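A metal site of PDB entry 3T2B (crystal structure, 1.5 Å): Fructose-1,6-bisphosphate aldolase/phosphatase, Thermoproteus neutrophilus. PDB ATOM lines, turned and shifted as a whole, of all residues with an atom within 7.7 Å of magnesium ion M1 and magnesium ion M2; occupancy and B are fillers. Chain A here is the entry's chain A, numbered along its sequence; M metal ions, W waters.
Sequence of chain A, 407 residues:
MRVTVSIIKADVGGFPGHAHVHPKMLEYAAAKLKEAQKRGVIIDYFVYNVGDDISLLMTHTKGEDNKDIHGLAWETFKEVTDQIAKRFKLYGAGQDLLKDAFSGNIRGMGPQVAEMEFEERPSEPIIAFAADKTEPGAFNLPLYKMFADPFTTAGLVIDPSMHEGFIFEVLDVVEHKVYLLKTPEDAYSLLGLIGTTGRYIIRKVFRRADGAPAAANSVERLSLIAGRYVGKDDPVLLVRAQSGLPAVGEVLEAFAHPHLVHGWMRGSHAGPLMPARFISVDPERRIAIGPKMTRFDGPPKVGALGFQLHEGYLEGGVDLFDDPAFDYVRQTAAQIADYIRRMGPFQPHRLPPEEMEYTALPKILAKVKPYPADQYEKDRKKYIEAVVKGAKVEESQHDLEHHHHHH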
ATOM      1  N   LYS A   9      -7.050  -9.550   2.593  1.00  0.00           N
ATOM      2  CA  LYS A   9      -6.451 -10.364   1.503  1.00  0.00           C
ATOM      3  C   LYS A   9      -6.008  -9.412   0.385  1.00  0.00           C
ATOM      4  O   LYS A   9      -6.626  -8.417   0.119  1.00  0.00           O
ATOM      5  CB  LYS A   9      -7.622 -11.265   1.047  1.00  0.00           C
ATOM      6  CG  LYS A   9      -7.326 -12.181  -0.235  1.00  0.00           C
ATOM      7  CD  LYS A   9      -8.199 -11.785  -1.405  1.00  0.00           C
ATOM      8  CE  LYS A   9      -7.600 -10.711  -2.212  1.00  0.00           C
ATOM      9  NZ  LYS A   9      -8.295 -10.487  -3.563  1.00  0.00           N
ATOM     10  N   ALA A  10      -4.930  -9.777  -0.269  1.00  0.00           N
ATOM     11  CA  ALA A  10      -4.476  -8.977  -1.403  1.00  0.00           C
ATOM     12  C   ALA A  10      -3.698  -9.866  -2.317  1.00  0.00           C
ATOM     13  O   ALA A  10      -3.055 -10.886  -1.873  1.00  0.00           O
ATOM     14  CB  ALA A  10      -3.533  -7.742  -0.939  1.00  0.00           C
ATOM     15  N   ASP A  11      -3.656  -9.421  -3.569  1.00  0.00           N
ATOM     16  CA  ASP A  11      -2.705 -10.054  -4.523  1.00  0.00           C
ATOM     17  C   ASP A  11      -1.580  -9.027  -4.811  1.00  0.00           C
ATOM     18  O   ASP A  11      -1.865  -7.993  -5.463  1.00  0.00           O
ATOM     19  CB  ASP A  11      -3.541 -10.290  -5.776  1.00  0.00           C
ATOM     20  CG  ASP A  11      -2.718 -10.832  -6.965  1.00  0.00           C
ATOM     21  OD1 ASP A  11      -1.492 -10.813  -7.058  1.00  0.00           O
ATOM     22  OD2 ASP A  11      -3.410 -11.226  -7.951  1.00  0.00           O
ATOM     23  N   VAL A  12      -0.397  -9.298  -4.362  1.00  0.00           N
ATOM     24  CA  VAL A  12       0.716  -8.373  -4.617  1.00  0.00           C
ATOM     25  C   VAL A  12       1.748  -9.053  -5.428  1.00  0.00           C
ATOM     26  O   VAL A  12       2.903  -8.688  -5.472  1.00  0.00           O
ATOM     27  CB  VAL A  12       1.351  -7.814  -3.288  1.00  0.00           C
ATOM     28  CG1 VAL A  12       0.267  -7.050  -2.435  1.00  0.00           C
ATOM     29  CG2 VAL A  12       1.958  -8.896  -2.454  1.00  0.00           C
ATOM     30  N   GLY A  13       1.326 -10.083  -6.177  1.00  0.00           N
ATOM     31  CA  GLY A  13       2.261 -10.631  -7.173  1.00  0.00           C
ATOM     32  C   GLY A  13       2.050 -12.121  -7.306  1.00  0.00           C
ATOM     33  O   GLY A  13       1.903 -12.841  -6.351  1.00  0.00           O
ATOM     34  N   GLY A  14       2.129 -12.576  -8.550  1.00  0.00           N
ATOM     35  CA  GLY A  14       1.818 -14.013  -8.839  1.00  0.00           C
ATOM     36  C   GLY A  14       3.057 -14.686  -9.385  1.00  0.00           C
ATOM     37  O   GLY A  14       4.066 -14.052  -9.864  1.00  0.00           O
ATOM     38  N   PHE A  15       2.972 -16.003  -9.437  1.00  0.00           N
ATOM     39  CA  PHE A  15       4.162 -16.819  -9.533  1.00  0.00           C
ATOM     40  C   PHE A  15       3.811 -18.197 -10.194  1.00  0.00           C
ATOM     41  O   PHE A  15       3.522 -19.134  -9.472  1.00  0.00           O
ATOM     42  CB  PHE A  15       4.785 -17.066  -8.163  1.00  0.00           C
ATOM     43  CG  PHE A  15       6.046 -17.872  -8.169  1.00  0.00           C
ATOM     44  CD1 PHE A  15       7.111 -17.507  -9.025  1.00  0.00           C
ATOM     45  CD2 PHE A  15       6.174 -18.925  -7.336  1.00  0.00           C
ATOM     46  CE1 PHE A  15       8.289 -18.269  -9.038  1.00  0.00           C
ATOM     47  CE2 PHE A  15       7.348 -19.735  -7.294  1.00  0.00           C
ATOM     48  CZ  PHE A  15       8.405 -19.361  -8.142  1.00  0.00           C
ATOM     49  N   GLY A  17       2.635 -15.499 -13.474  1.00  0.00           N
ATOM     50  CA  GLY A  17       1.379 -14.976 -13.907  1.00  0.00           C
ATOM     51  C   GLY A  17       0.460 -14.825 -12.769  1.00  0.00           C
ATOM     52  O   GLY A  17       0.792 -14.230 -11.709  1.00  0.00           O
ATOM     53  N   HIS A  18      -0.767 -15.329 -12.924  1.00  0.00           N
ATOM     54  CA  HIS A  18      -1.736 -15.310 -11.795  1.00  0.00           C
ATOM     55  C   HIS A  18      -1.964 -16.716 -11.238  1.00  0.00           C
ATOM     56  O   HIS A  18      -3.005 -16.991 -10.630  1.00  0.00           O
ATOM     57  CB  HIS A  18      -3.059 -14.732 -12.275  1.00  0.00           C
ATOM     58  CG  HIS A  18      -2.914 -13.411 -12.949  1.00  0.00           C
ATOM     59  ND1 HIS A  18      -2.835 -12.253 -12.193  1.00  0.00           N
ATOM     60  CD2 HIS A  18      -2.952 -13.034 -14.240  1.00  0.00           C
ATOM     61  CE1 HIS A  18      -2.784 -11.216 -13.021  1.00  0.00           C
ATOM     62  NE2 HIS A  18      -2.864 -11.652 -14.281  1.00  0.00           N
ATOM     63  N   ALA A  19      -0.968 -17.565 -11.404  1.00  0.00           N
ATOM     64  CA  ALA A  19      -1.235 -18.993 -11.076  1.00  0.00           C
ATOM     65  C   ALA A  19      -1.125 -19.345  -9.617  1.00  0.00           C
ATOM     66  O   ALA A  19      -1.671 -20.359  -9.139  1.00  0.00           O
ATOM     67  CB  ALA A  19      -0.252 -19.909 -11.915  1.00  0.00           C
ATOM     68  N   HIS A  20      -0.264 -18.625  -8.843  1.00  0.00           N
ATOM     69  CA  HIS A  20       0.089 -19.101  -7.514  1.00  0.00           C
ATOM     70  C   HIS A  20       0.830 -17.892  -6.841  1.00  0.00           C
ATOM     71  O   HIS A  20       0.888 -16.820  -7.487  1.00  0.00           O
ATOM     72  CB  HIS A  20       0.999 -20.296  -7.572  1.00  0.00           C
ATOM     73  CG  HIS A  20       0.772 -21.255  -6.433  1.00  0.00           C
ATOM     74  ND1 HIS A  20       1.782 -22.057  -5.939  1.00  0.00           N
ATOM     75  CD2 HIS A  20      -0.363 -21.617  -5.790  1.00  0.00           C
ATOM     76  CE1 HIS A  20       1.278 -22.858  -4.991  1.00  0.00           C
ATOM     77  NE2 HIS A  20      -0.031 -22.605  -4.876  1.00  0.00           N
ATOM     78  N   VAL A  50      -4.874 -18.820  -1.790  1.00  0.00           N
ATOM     79  CA  VAL A  50      -5.567 -19.737  -2.791  1.00  0.00           C
ATOM     80  C   VAL A  50      -5.241 -19.014  -4.087  1.00  0.00           C
ATOM     81  O   VAL A  50      -5.506 -17.815  -4.327  1.00  0.00           O
ATOM     82  CB  VAL A  50      -7.064 -19.785  -2.514  1.00  0.00           C
ATOM     83  CG1 VAL A  50      -7.854 -20.471  -3.768  1.00  0.00           C
ATOM     84  CG2 VAL A  50      -7.393 -20.569  -1.213  1.00  0.00           C
ATOM     85  N   GLY A  51      -4.568 -19.771  -5.006  1.00  0.00           N
ATOM     86  CA  GLY A  51      -4.147 -19.047  -6.258  1.00  0.00           C
ATOM     87  C   GLY A  51      -3.130 -17.939  -5.936  1.00  0.00           C
ATOM     88  O   GLY A  51      -2.241 -18.164  -5.164  1.00  0.00           O
ATOM     89  N   ASP A  52      -3.382 -16.858  -6.597  1.00  0.00           N
ATOM     90  CA  ASP A  52      -2.439 -15.713  -6.426  1.00  0.00           C
ATOM     91  C   ASP A  52      -2.866 -14.724  -5.334  1.00  0.00           C
ATOM     92  O   ASP A  52      -2.301 -13.603  -5.330  1.00  0.00           O
ATOM     93  CB  ASP A  52      -2.267 -15.024  -7.776  1.00  0.00           C
ATOM     94  CG  ASP A  52      -3.551 -14.380  -8.296  1.00  0.00           C
ATOM     95  OD1 ASP A  52      -4.673 -14.583  -7.756  1.00  0.00           O
ATOM     96  OD2 ASP A  52      -3.500 -13.687  -9.386  1.00  0.00           O
ATOM     97  N   ASP A  53      -3.783 -15.060  -4.479  1.00  0.00           N
ATOM     98  CA  ASP A  53      -4.240 -14.178  -3.380  1.00  0.00           C
ATOM     99  C   ASP A  53      -3.781 -14.651  -2.023  1.00  0.00           C
ATOM    100  O   ASP A  53      -4.017 -15.813  -1.602  1.00  0.00           O
ATOM    101  CB  ASP A  53      -5.738 -14.020  -3.373  1.00  0.00           C
ATOM    102  CG  ASP A  53      -6.237 -13.382  -4.611  1.00  0.00           C
ATOM    103  OD1 ASP A  53      -6.270 -12.150  -4.715  1.00  0.00           O
ATOM    104  OD2 ASP A  53      -6.537 -14.148  -5.573  1.00  0.00           O
ATOM    105  N   ILE A  54      -3.130 -13.709  -1.262  1.00  0.00           N
ATOM    106  CA  ILE A  54      -2.681 -14.048   0.148  1.00  0.00           C
ATOM    107  C   ILE A  54      -3.692 -13.485   1.139  1.00  0.00           C
ATOM    108  O   ILE A  54      -4.074 -12.290   1.037  1.00  0.00           O
ATOM    109  CB  ILE A  54      -1.367 -13.377   0.405  1.00  0.00           C
ATOM    110  CG1 ILE A  54      -0.381 -14.104  -0.517  1.00  0.00           C
ATOM    111  CG2 ILE A  54      -0.966 -13.577   1.902  1.00  0.00           C
ATOM    112  CD1 ILE A  54       1.138 -13.561  -0.492  1.00  0.00           C
ATOM    113  N   TYR A  91       4.434 -11.327 -11.274  1.00  0.00           N
ATOM    114  CA  TYR A  91       3.508 -10.700 -12.179  1.00  0.00           C
ATOM    115  C   TYR A  91       2.380 -10.045 -11.453  1.00  0.00           C
ATOM    116  O   TYR A  91       1.724 -10.646 -10.589  1.00  0.00           O
ATOM    117  CB  TYR A  91       2.922 -11.870 -13.171  1.00  0.00           C
ATOM    118  CG  TYR A  91       2.216 -11.205 -14.297  1.00  0.00           C
ATOM    119  CD1 TYR A  91       2.898 -10.717 -15.412  1.00  0.00           C
ATOM    120  CD2 TYR A  91       0.874 -10.938 -14.193  1.00  0.00           C
ATOM    121  CE1 TYR A  91       2.243  -9.993 -16.421  1.00  0.00           C
ATOM    122  CE2 TYR A  91       0.215 -10.225 -15.193  1.00  0.00           C
ATOM    123  CZ  TYR A  91       0.922  -9.760 -16.267  1.00  0.00           C
ATOM    124  OH  TYR A  91       0.120  -9.028 -17.185  1.00  0.00           O
ATOM    125  N   GLY A  92       2.125  -8.790 -11.793  1.00  0.00           N
ATOM    126  CA  GLY A  92       1.165  -7.935 -11.015  1.00  0.00           C
ATOM    127  C   GLY A  92       1.778  -7.492  -9.686  1.00  0.00           C
ATOM    128  O   GLY A  92       1.081  -7.166  -8.731  1.00  0.00           O
ATOM    129  N   ALA A  93       3.117  -7.460  -9.596  1.00  0.00           N
ATOM    130  CA  ALA A  93       3.799  -7.049  -8.331  1.00  0.00           C
ATOM    131  C   ALA A  93       3.148  -5.749  -7.752  1.00  0.00           C
ATOM    132  O   ALA A  93       3.004  -4.731  -8.451  1.00  0.00           O
ATOM    133  CB  ALA A  93       5.350  -6.824  -8.567  1.00  0.00           C
ATOM    134  N   GLN A  95       0.272  -4.856  -7.085  1.00  0.00           N
ATOM    135  CA  GLN A  95      -0.813  -4.145  -7.790  1.00  0.00           C
ATOM    136  C   GLN A  95      -2.110  -3.917  -7.022  1.00  0.00           C
ATOM    137  O   GLN A  95      -2.905  -3.079  -7.441  1.00  0.00           O
ATOM    138  CB  GLN A  95      -1.182  -4.756  -9.151  1.00  0.00           C
ATOM    139  CG  GLN A  95      -1.164  -3.703 -10.263  1.00  0.00           C
ATOM    140  CD  GLN A  95      -0.040  -3.979 -11.261  1.00  0.00           C
ATOM    141  OE1 GLN A  95       1.098  -3.483 -11.121  1.00  0.00           O
ATOM    142  NE2 GLN A  95      -0.348  -4.821 -12.272  1.00  0.00           N
ATOM    143  N   ASP A  96      -2.356  -4.670  -5.942  1.00  0.00           N
ATOM    144  CA  ASP A  96      -3.549  -4.367  -5.117  1.00  0.00           C
ATOM    145  C   ASP A  96      -3.334  -3.134  -4.243  1.00  0.00           C
ATOM    146  O   ASP A  96      -4.296  -2.670  -3.659  1.00  0.00           O
ATOM    147  CB  ASP A  96      -3.963  -5.553  -4.231  1.00  0.00           C
ATOM    148  CG  ASP A  96      -4.986  -6.450  -4.902  1.00  0.00           C
ATOM    149  OD1 ASP A  96      -5.411  -6.139  -6.048  1.00  0.00           O
ATOM    150  OD2 ASP A  96      -5.385  -7.478  -4.292  1.00  0.00           O
ATOM    151  N   ALA A 131     -11.494 -17.554  -2.201  1.00  0.00           N
ATOM    152  CA  ALA A 131     -11.726 -18.010  -3.625  1.00  0.00           C
ATOM    153  C   ALA A 131     -10.814 -17.279  -4.515  1.00  0.00           C
ATOM    154  O   ALA A 131     -10.479 -16.103  -4.241  1.00  0.00           O
ATOM    155  CB  ALA A 131     -13.119 -17.837  -4.000  1.00  0.00           C
ATOM    156  N   ASP A 132     -10.277 -17.877  -5.559  1.00  0.00           N
ATOM    157  CA  ASP A 132      -9.481 -17.099  -6.481  1.00  0.00           C
ATOM    158  C   ASP A 132     -10.224 -17.222  -7.843  1.00  0.00           C
ATOM    159  O   ASP A 132     -10.983 -18.184  -8.114  1.00  0.00           O
ATOM    160  CB  ASP A 132      -8.093 -17.746  -6.606  1.00  0.00           C
ATOM    161  CG  ASP A 132      -7.164 -16.983  -7.530  1.00  0.00           C
ATOM    162  OD1 ASP A 132      -7.396 -15.753  -7.706  1.00  0.00           O
ATOM    163  OD2 ASP A 132      -6.149 -17.510  -7.994  1.00  0.00           O
ATOM    164  N   LYS A 133      -9.969 -16.238  -8.687  1.00  0.00           N
ATOM    165  CA  LYS A 133     -10.531 -16.151 -10.037  1.00  0.00           C
ATOM    166  C   LYS A 133     -11.993 -16.008 -10.055  1.00  0.00           C
ATOM    167  O   LYS A 133     -12.723 -16.557 -10.956  1.00  0.00           O
ATOM    168  CB  LYS A 133      -9.994 -17.361 -10.916  1.00  0.00           C
ATOM    169  CG  LYS A 133      -8.469 -17.469 -10.874  1.00  0.00           C
ATOM    170  CD  LYS A 133      -7.753 -16.360 -11.643  1.00  0.00           C
ATOM    171  CE  LYS A 133      -6.279 -16.527 -11.718  1.00  0.00           C
ATOM    172  NZ  LYS A 133      -5.674 -16.146 -10.374  1.00  0.00           N
ATOM    173  N   THR A 134     -12.581 -15.254  -9.112  1.00  0.00           N
ATOM    174  CA  THR A 134     -14.012 -14.969  -9.084  1.00  0.00           C
ATOM    175  C   THR A 134     -14.291 -13.687  -8.333  1.00  0.00           C
ATOM    176  O   THR A 134     -13.366 -13.012  -7.951  1.00  0.00           O
ATOM    177  CB  THR A 134     -14.816 -16.156  -8.460  1.00  0.00           C
ATOM    178  OG1 THR A 134     -14.801 -16.108  -7.004  1.00  0.00           O
ATOM    179  CG2 THR A 134     -14.123 -17.372  -8.815  1.00  0.00           C
ATOM    180  N   ASP A 233     -12.716  -7.861  -7.017  1.00  0.00           N
ATOM    181  CA  ASP A 233     -11.599  -8.607  -6.614  1.00  0.00           C
ATOM    182  C   ASP A 233     -11.968  -9.938  -5.894  1.00  0.00           C
ATOM    183  O   ASP A 233     -12.988 -10.072  -5.224  1.00  0.00           O
ATOM    184  CB  ASP A 233     -10.704  -7.727  -5.667  1.00  0.00           C
ATOM    185  CG  ASP A 233     -10.585  -6.207  -6.184  1.00  0.00           C
ATOM    186  OD1 ASP A 233      -9.619  -5.993  -6.875  1.00  0.00           O
ATOM    187  OD2 ASP A 233     -11.517  -5.380  -5.909  1.00  0.00           O
ATOM    188  N   ASP A 234     -11.012 -10.850  -5.970  1.00  0.00           N
ATOM    189  CA  ASP A 234     -11.260 -12.254  -5.489  1.00  0.00           C
ATOM    190  C   ASP A 234     -11.573 -12.217  -4.001  1.00  0.00           C
ATOM    191  O   ASP A 234     -10.863 -11.473  -3.187  1.00  0.00           O
ATOM    192  CB  ASP A 234     -10.016 -13.098  -5.698  1.00  0.00           C
ATOM    193  CG  ASP A 234      -9.563 -13.231  -7.189  1.00  0.00           C
ATOM    194  OD1 ASP A 234     -10.469 -13.205  -7.976  1.00  0.00           O
ATOM    195  OD2 ASP A 234      -8.356 -13.191  -7.518  1.00  0.00           O
ATOM    196  N   PRO A 235     -12.648 -12.869  -3.597  1.00  0.00           N
ATOM    197  CA  PRO A 235     -13.178 -12.678  -2.244  1.00  0.00           C
ATOM    198  C   PRO A 235     -12.669 -13.580  -1.169  1.00  0.00           C
ATOM    199  O   PRO A 235     -12.080 -14.633  -1.389  1.00  0.00           O
ATOM    200  CB  PRO A 235     -14.653 -12.853  -2.396  1.00  0.00           C
ATOM    201  CG  PRO A 235     -14.728 -14.054  -3.499  1.00  0.00           C
ATOM    202  CD  PRO A 235     -13.640 -13.590  -4.468  1.00  0.00           C
ATOM    203  N   MET A 293      -3.777 -22.122  -9.986  1.00  0.00           N
ATOM    204  CA  MET A 293      -4.699 -21.926 -11.096  1.00  0.00           C
ATOM    205  C   MET A 293      -3.915 -22.265 -12.348  1.00  0.00           C
ATOM    206  O   MET A 293      -2.792 -21.806 -12.583  1.00  0.00           O
ATOM    207  CB  MET A 293      -5.201 -20.468 -11.191  1.00  0.00           C
ATOM    208  CG  MET A 293      -5.785 -19.963  -9.866  1.00  0.00           C
ATOM    209  SD  MET A 293      -7.185 -20.963  -9.292  1.00  0.00           S
ATOM    210  CE  MET A 293      -6.657 -21.340  -7.753  1.00  0.00           C
HETATM  211 MG    MG M   1      -6.565 -13.892  -7.637  1.00  0.00          MG
HETATM  212 MG    MG M   2      -3.022 -11.805  -9.972  1.00  0.00          MG
HETATM  213  O   HOH W   1      -2.600  -9.691 -10.271  1.00  0.00           O
HETATM  214  O   HOH W   2      -6.613 -13.566  -9.661  1.00  0.00           O
HETATM  215  O   HOH W   3      -1.027 -11.948  -9.526  1.00  0.00           O
HETATM  216  O   HOH W   4      -6.006 -11.902  -7.298  1.00  0.00           O
HETATM  217  O   HOH W   5      -5.005 -11.307 -10.346  1.00  0.00           O
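OD2 of Asp 52 binds magnesium ion M2, at 2.0 Å.
Water W3 binds magnesium ion M2 (2.0 Å).
Magnesium ion M2 is bound by water W5.
Magnesium ion M2 is bound by OD2 of Asp 11 (2.1 Å).
Magnesium ion M2 is bound by water W1 (2.2 Å).
A ring nitrogen (ND1) of His 18 binds magnesium ion M2.
Magnesium ion M2 has six donor atoms within binding distance.
Water W3 lies within hydrogen-bond range of OD1 of Asp 11 (2.8 Å), O of Tyr 91 (3.2 Å) and N of Gly 14 (3.4 Å).
Magnesium ion M1 is bound by the side-chain carboxylate (OD2) of Asp 234 (1.9 Å), the side-chain carboxylate (OD1) of Asp 52 (2.0 Å), the side-chain carboxylate (OD1) of Asp 132 (2.0 Å), water W2 (2.1 Å), the side-chain carboxylate (OD2) of Asp 53 (2.1 Å) and water W4 (2.1 Å).
NZ of Lys 133 touches magnesium ion M1 (3.7 Å).
Of the 29 residues printed, 3 come within 4 Å of magnesium ion M2.
OD1 of Asp 53 is in salt-bridge range of NZ of Lys 9 (2.9 Å).
The backbone carbonyl oxygen (O) of Asp 234 sits at hydrogen-bond distance from the side-chain amino group (NZ) of Lys 9, at 2.8 Å.
N of Asp 11 sits at hydrogen-bond distance from OD2 of Asp 96.
OD1 of Asp 52 sits close to NZ of Lys 133 (3.2 Å).
The side-chain carboxylate (OD1) of Asp 234 sits at hydrogen-bond distance from the backbone NH (N) of Thr 134.
OD2 of Asp 132 lies within salt-bridge range of NZ of Lys 133 (2.8 Å).
O of His 18 sits at hydrogen-bond distance from NZ of Lys 133 (2.8 Å).
OD1 of Asp 11 is in hydrogen-bond range of N of Gly 13, at 3.0 Å.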
